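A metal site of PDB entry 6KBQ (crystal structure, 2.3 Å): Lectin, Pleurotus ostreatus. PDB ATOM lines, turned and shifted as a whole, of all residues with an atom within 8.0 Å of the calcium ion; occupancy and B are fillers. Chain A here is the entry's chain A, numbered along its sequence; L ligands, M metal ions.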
ATOM      1  N   TRP A  57     -22.533   1.259  -8.074  1.00  0.00           N
ATOM      2  CA  TRP A  57     -21.191   1.714  -7.762  1.00  0.00           C
ATOM      3  C   TRP A  57     -20.832   1.098  -6.424  1.00  0.00           C
ATOM      4  O   TRP A  57     -21.414   0.068  -6.051  1.00  0.00           O
ATOM      5  CB  TRP A  57     -21.088   3.261  -7.721  1.00  0.00           C
ATOM      6  CG  TRP A  57     -19.666   3.758  -7.849  1.00  0.00           C
ATOM      7  CD1 TRP A  57     -18.946   4.481  -6.916  1.00  0.00           C
ATOM      8  CD2 TRP A  57     -18.755   3.544  -8.954  1.00  0.00           C
ATOM      9  NE1 TRP A  57     -17.678   4.732  -7.388  1.00  0.00           N
ATOM     10  CE2 TRP A  57     -17.530   4.161  -8.625  1.00  0.00           C
ATOM     11  CE3 TRP A  57     -18.875   2.890 -10.189  1.00  0.00           C
ATOM     12  CZ2 TRP A  57     -16.434   4.151  -9.496  1.00  0.00           C
ATOM     13  CZ3 TRP A  57     -17.780   2.874 -11.052  1.00  0.00           C
ATOM     14  CH2 TRP A  57     -16.575   3.505 -10.700  1.00  0.00           C
ATOM     15  N   GLY A  66     -24.298  10.643  -5.882  1.00  0.00           N
ATOM     16  CA  GLY A  66     -23.510  11.664  -5.240  1.00  0.00           C
ATOM     17  C   GLY A  66     -22.100  11.726  -5.815  1.00  0.00           C
ATOM     18  O   GLY A  66     -21.695  10.938  -6.677  1.00  0.00           O
ATOM     19  N   ASN A  68     -18.231  11.401  -6.294  1.00  0.00           N
ATOM     20  CA  ASN A  68     -17.282  10.335  -6.024  1.00  0.00           C
ATOM     21  C   ASN A  68     -15.916  10.772  -6.525  1.00  0.00           C
ATOM     22  O   ASN A  68     -15.798  11.692  -7.338  1.00  0.00           O
ATOM     23  CB  ASN A  68     -17.701   9.036  -6.709  1.00  0.00           C
ATOM     24  CG  ASN A  68     -18.853   8.348  -5.986  1.00  0.00           C
ATOM     25  OD1 ASN A  68     -20.033   8.712  -6.154  1.00  0.00           O
ATOM     26  ND2 ASN A  68     -18.518   7.371  -5.178  1.00  0.00           N
ATOM     27  N   ILE A  69     -14.885  10.104  -6.014  1.00  0.00           N
ATOM     28  CA  ILE A  69     -13.520  10.433  -6.383  1.00  0.00           C
ATOM     29  C   ILE A  69     -13.167   9.771  -7.711  1.00  0.00           C
ATOM     30  O   ILE A  69     -13.790   8.784  -8.133  1.00  0.00           O
ATOM     31  CB  ILE A  69     -12.523   9.996  -5.289  1.00  0.00           C
ATOM     32  CG1 ILE A  69     -12.578   8.470  -5.136  1.00  0.00           C
ATOM     33  CG2 ILE A  69     -12.836  10.709  -3.966  1.00  0.00           C
ATOM     34  CD1 ILE A  69     -11.406   7.899  -4.304  1.00  0.00           C
ATOM     35  N   ILE A  70     -12.124  10.293  -8.364  1.00  0.00           N
ATOM     36  CA  ILE A  70     -11.519   9.592  -9.483  1.00  0.00           C
ATOM     37  C   ILE A  70     -10.976   8.254  -8.980  1.00  0.00           C
ATOM     38  O   ILE A  70     -10.234   8.196  -7.992  1.00  0.00           O
ATOM     39  CB  ILE A  70     -10.417  10.439 -10.131  1.00  0.00           C
ATOM     40  CG1 ILE A  70     -11.038  11.708 -10.729  1.00  0.00           C
ATOM     41  CG2 ILE A  70      -9.679   9.633 -11.218  1.00  0.00           C
ATOM     42  CD1 ILE A  70     -10.057  12.846 -10.962  1.00  0.00           C
ATOM     43  N   SER A  96     -22.026   3.494 -18.786  1.00  0.00           N
ATOM     44  CA  SER A  96     -21.133   3.803 -17.681  1.00  0.00           C
ATOM     45  C   SER A  96     -20.950   5.295 -17.506  1.00  0.00           C
ATOM     46  O   SER A  96     -20.921   6.060 -18.473  1.00  0.00           O
ATOM     47  CB  SER A  96     -19.748   3.168 -17.874  1.00  0.00           C
ATOM     48  OG  SER A  96     -19.172   3.634 -19.091  1.00  0.00           O
ATOM     49  N   ASP A  97     -20.778   5.696 -16.254  1.00  0.00           N
ATOM     50  CA  ASP A  97     -20.273   7.009 -15.914  1.00  0.00           C
ATOM     51  C   ASP A  97     -19.043   6.743 -15.054  1.00  0.00           C
ATOM     52  O   ASP A  97     -19.195   6.399 -13.878  1.00  0.00           O
ATOM     53  CB  ASP A  97     -21.333   7.828 -15.185  1.00  0.00           C
ATOM     54  CG  ASP A  97     -20.834   9.204 -14.765  1.00  0.00           C
ATOM     55  OD1 ASP A  97     -19.621   9.464 -14.910  1.00  0.00           O
ATOM     56  OD2 ASP A  97     -21.650  10.023 -14.296  1.00  0.00           O
ATOM     57  N   ASP A  98     -17.835   6.873 -15.622  1.00  0.00           N
ATOM     58  CA  ASP A  98     -17.586   7.429 -16.975  1.00  0.00           C
ATOM     59  C   ASP A  98     -17.223   6.402 -18.057  1.00  0.00           C
ATOM     60  O   ASP A  98     -17.481   6.626 -19.226  1.00  0.00           O
ATOM     61  CB  ASP A  98     -16.433   8.454 -16.929  1.00  0.00           C
ATOM     62  CG  ASP A  98     -16.747   9.669 -16.076  1.00  0.00           C
ATOM     63  OD1 ASP A  98     -17.315  10.653 -16.605  1.00  0.00           O
ATOM     64  OD2 ASP A  98     -16.396   9.660 -14.872  1.00  0.00           O
ATOM     65  N   ALA A  99     -16.579   5.290 -17.680  1.00  0.00           N
ATOM     66  CA  ALA A  99     -16.035   4.353 -18.650  1.00  0.00           C
ATOM     67  C   ALA A  99     -16.039   2.959 -18.052  1.00  0.00           C
ATOM     68  O   ALA A  99     -16.091   2.796 -16.830  1.00  0.00           O
ATOM     69  CB  ALA A  99     -14.599   4.733 -19.073  1.00  0.00           C
ATOM     70  N   PHE A 115     -22.945   7.485 -20.608  1.00  0.00           N
ATOM     71  CA  PHE A 115     -24.249   7.099 -20.083  1.00  0.00           C
ATOM     72  C   PHE A 115     -25.418   7.579 -20.926  1.00  0.00           C
ATOM     73  O   PHE A 115     -26.560   7.189 -20.647  1.00  0.00           O
ATOM     74  CB  PHE A 115     -24.409   7.627 -18.648  1.00  0.00           C
ATOM     75  CG  PHE A 115     -24.255   9.143 -18.521  1.00  0.00           C
ATOM     76  CD1 PHE A 115     -25.363   9.978 -18.691  1.00  0.00           C
ATOM     77  CD2 PHE A 115     -23.025   9.709 -18.195  1.00  0.00           C
ATOM     78  CE1 PHE A 115     -25.223  11.358 -18.549  1.00  0.00           C
ATOM     79  CE2 PHE A 115     -22.883  11.078 -18.062  1.00  0.00           C
ATOM     80  CZ  PHE A 115     -23.974  11.909 -18.246  1.00  0.00           C
ATOM     81  N   GLN A 137     -14.832   3.064 -14.205  1.00  0.00           N
ATOM     82  CA  GLN A 137     -13.929   4.156 -13.857  1.00  0.00           C
ATOM     83  C   GLN A 137     -14.701   5.461 -13.746  1.00  0.00           C
ATOM     84  O   GLN A 137     -15.428   5.836 -14.676  1.00  0.00           O
ATOM     85  CB  GLN A 137     -12.827   4.384 -14.894  1.00  0.00           C
ATOM     86  CG  GLN A 137     -11.969   3.192 -15.279  1.00  0.00           C
ATOM     87  CD  GLN A 137     -11.114   3.539 -16.510  1.00  0.00           C
ATOM     88  OE1 GLN A 137     -10.509   4.615 -16.567  1.00  0.00           O
ATOM     89  NE2 GLN A 137     -11.081   2.639 -17.500  1.00  0.00           N
ATOM     90  N   ASN A 138     -14.509   6.154 -12.641  1.00  0.00           N
ATOM     91  CA  ASN A 138     -14.922   7.543 -12.520  1.00  0.00           C
ATOM     92  C   ASN A 138     -13.739   8.427 -12.917  1.00  0.00           C
ATOM     93  O   ASN A 138     -12.643   8.291 -12.358  1.00  0.00           O
ATOM     94  CB  ASN A 138     -15.380   7.847 -11.100  1.00  0.00           C
ATOM     95  CG  ASN A 138     -16.011   9.206 -10.992  1.00  0.00           C
ATOM     96  OD1 ASN A 138     -16.499   9.741 -11.994  1.00  0.00           O
ATOM     97  ND2 ASN A 138     -15.980   9.796  -9.796  1.00  0.00           N
ATOM     98  N   LEU A 139     -13.957   9.315 -13.890  1.00  0.00           N
ATOM     99  CA  LEU A 139     -12.850  10.069 -14.445  1.00  0.00           C
ATOM    100  C   LEU A 139     -12.888  11.549 -14.123  1.00  0.00           C
ATOM    101  O   LEU A 139     -11.908  12.243 -14.402  1.00  0.00           O
ATOM    102  CB  LEU A 139     -12.792   9.882 -15.974  1.00  0.00           C
ATOM    103  CG  LEU A 139     -12.423   8.464 -16.426  1.00  0.00           C
ATOM    104  CD1 LEU A 139     -12.608   8.281 -17.928  1.00  0.00           C
ATOM    105  CD2 LEU A 139     -10.981   8.115 -16.042  1.00  0.00           C
ATOM    106  N   VAL A 140     -13.964  12.056 -13.527  1.00  0.00           N
ATOM    107  CA  VAL A 140     -14.079  13.455 -13.151  1.00  0.00           C
ATOM    108  C   VAL A 140     -14.247  13.536 -11.647  1.00  0.00           C
ATOM    109  O   VAL A 140     -15.095  12.833 -11.069  1.00  0.00           O
ATOM    110  CB  VAL A 140     -15.259  14.129 -13.872  1.00  0.00           C
ATOM    111  CG1 VAL A 140     -15.368  15.577 -13.428  1.00  0.00           C
ATOM    112  CG2 VAL A 140     -15.088  14.038 -15.385  1.00  0.00           C
ATOM    113  N   ALA A 141     -13.455  14.394 -10.997  1.00  0.00           N
ATOM    114  CA  ALA A 141     -13.521  14.517  -9.550  1.00  0.00           C
ATOM    115  C   ALA A 141     -14.857  15.115  -9.106  1.00  0.00           C
ATOM    116  O   ALA A 141     -15.464  15.922  -9.815  1.00  0.00           O
ATOM    117  CB  ALA A 141     -12.363  15.384  -9.045  1.00  0.00           C
ATOM    118  N   ASN A 142     -15.335  14.696  -7.929  1.00  0.00           N
ATOM    119  CA  ASN A 142     -16.570  15.230  -7.343  1.00  0.00           C
ATOM    120  C   ASN A 142     -17.792  14.987  -8.223  1.00  0.00           C
ATOM    121  O   ASN A 142     -18.761  15.739  -8.183  1.00  0.00           O
ATOM    122  CB  ASN A 142     -16.482  16.741  -7.058  1.00  0.00           C
ATOM    123  CG  ASN A 142     -15.307  17.110  -6.209  1.00  0.00           C
ATOM    124  OD1 ASN A 142     -15.049  16.476  -5.175  1.00  0.00           O
ATOM    125  ND2 ASN A 142     -14.562  18.118  -6.634  1.00  0.00           N
ATOM    126  N   SER A 143     -17.755  13.961  -9.069  1.00  0.00           N
ATOM    127  CA  SER A 143     -18.845  13.728 -10.004  1.00  0.00           C
ATOM    128  C   SER A 143     -19.459  12.365  -9.743  1.00  0.00           C
ATOM    129  O   SER A 143     -18.817  11.482  -9.147  1.00  0.00           O
ATOM    130  CB  SER A 143     -18.326  13.809 -11.447  1.00  0.00           C
ATOM    131  OG  SER A 143     -17.693  12.595 -11.813  1.00  0.00           O
ATOM    132  N   PRO A 144     -20.701  12.137 -10.180  1.00  0.00           N
ATOM    133  CA  PRO A 144     -21.321  10.821  -9.946  1.00  0.00           C
ATOM    134  C   PRO A 144     -20.564   9.719 -10.675  1.00  0.00           C
ATOM    135  O   PRO A 144     -19.756   9.964 -11.578  1.00  0.00           O
ATOM    136  CB  PRO A 144     -22.748  10.984 -10.484  1.00  0.00           C
ATOM    137  CG  PRO A 144     -22.774  12.248 -11.249  1.00  0.00           C
ATOM    138  CD  PRO A 144     -21.623  13.105 -10.779  1.00  0.00           C
ATOM    139  N   ALA A 145     -20.808   8.483 -10.249  1.00  0.00           N
ATOM    140  CA  ALA A 145     -20.164   7.309 -10.843  1.00  0.00           C
ATOM    141  C   ALA A 145     -21.153   6.152 -10.862  1.00  0.00           C
ATOM    142  O   ALA A 145     -21.945   5.993  -9.925  1.00  0.00           O
ATOM    143  CB  ALA A 145     -18.900   6.913 -10.075  1.00  0.00           C
ATOM    144  N   GLY A 146     -21.101   5.338 -11.908  1.00  0.00           N
ATOM    145  CA  GLY A 146     -21.977   4.181 -11.953  1.00  0.00           C
ATOM    146  C   GLY A 146     -21.874   3.406 -13.249  1.00  0.00           C
ATOM    147  O   GLY A 146     -21.417   3.924 -14.279  1.00  0.00           O
ATOM    148  N   TRP A 204     -28.745  10.182 -14.131  1.00  0.00           N
ATOM    149  CA  TRP A 204     -28.390  10.072 -15.545  1.00  0.00           C
ATOM    150  C   TRP A 204     -29.586  10.120 -16.492  1.00  0.00           C
ATOM    151  O   TRP A 204     -29.400  10.471 -17.657  1.00  0.00           O
ATOM    152  CB  TRP A 204     -27.611   8.762 -15.763  1.00  0.00           C
ATOM    153  CG  TRP A 204     -26.356   8.788 -14.970  1.00  0.00           C
ATOM    154  CD1 TRP A 204     -25.212   9.508 -15.246  1.00  0.00           C
ATOM    155  CD2 TRP A 204     -26.111   8.104 -13.730  1.00  0.00           C
ATOM    156  NE1 TRP A 204     -24.270   9.295 -14.260  1.00  0.00           N
ATOM    157  CE2 TRP A 204     -24.795   8.451 -13.315  1.00  0.00           C
ATOM    158  CE3 TRP A 204     -26.866   7.232 -12.929  1.00  0.00           C
ATOM    159  CZ2 TRP A 204     -24.226   7.947 -12.146  1.00  0.00           C
ATOM    160  CZ3 TRP A 204     -26.295   6.741 -11.775  1.00  0.00           C
ATOM    161  CH2 TRP A 204     -24.987   7.095 -11.394  1.00  0.00           C
HETATM  162  C1  LIG L   1     -21.479  13.802 -14.966  1.00  0.00           C
HETATM  163  O1  LIG L   1     -21.399  14.495 -16.172  1.00  0.00           O
HETATM  164  C2  LIG L   1     -20.344  12.742 -14.957  1.00  0.00           C
HETATM  165  O2  LIG L   1     -20.179  12.150 -13.715  1.00  0.00           O
HETATM  166  C3  LIG L   1     -19.048  13.452 -15.461  1.00  0.00           C
HETATM  167  O3  LIG L   1     -17.972  12.599 -15.153  1.00  0.00           O
HETATM  168 CA    CA M   1     -18.272  10.632 -13.366  1.00  0.00          CA
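N of Asp 97 is in hydrogen-bond range of O of Gly 146 (2.7 Å).
The indole nitrogen (NE1) of Trp 204 lies within hydrogen-bond range of the side-chain carboxylate (OD2) of Asp 97, at 2.7 Å.
O of Asn 68 lies within hydrogen-bond range of ND2 of Asn 138, 3.1 Å away.
The side-chain amide nitrogen (ND2) of Asn 138 is in hydrogen-bond range of the backbone carbonyl oxygen (O) of Ile 69 (2.9 Å).
The backbone carbonyl oxygen (O) of Val 140 sits close to the side-chain hydroxyl (OG) of Ser 143, 2.7 Å away.
The backbone NH of Asn 68 sits at hydrogen-bond distance from the backbone carbonyl oxygen of Ser 143 (2.9 Å).
The backbone carbonyl oxygen (O) of Gln 137 is in hydrogen-bond range of the backbone NH (N) of Asp 98 (2.8 Å).
The backbone carbonyl oxygen (O) of Asp 98 sits at hydrogen-bond distance from the side-chain hydroxyl (OG) of Ser 96 (3.4 Å).
Of the 21 residues printed, 5 come within 4 Å of the calcium ion.
The calcium ion is bound by OD1 of Asp 97 (2.4 Å).
The calcium ion is bound by OD1 of Asn 138, 2.4 Å away.
The calcium ion is bound by O of Pro 144, 2.4 Å away.
An oxygen (O2) of the ligand is bound to the calcium ion (2.5 Å).
OG of Ser 143 is bound to the calcium ion (2.6 Å).
The side-chain carboxylate (OD2) of Asp 98 is bound to the calcium ion.
The calcium ion is bound by O3 of the ligand, at 2.7 Å.
The calcium ion has seven donor atoms within binding distance.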
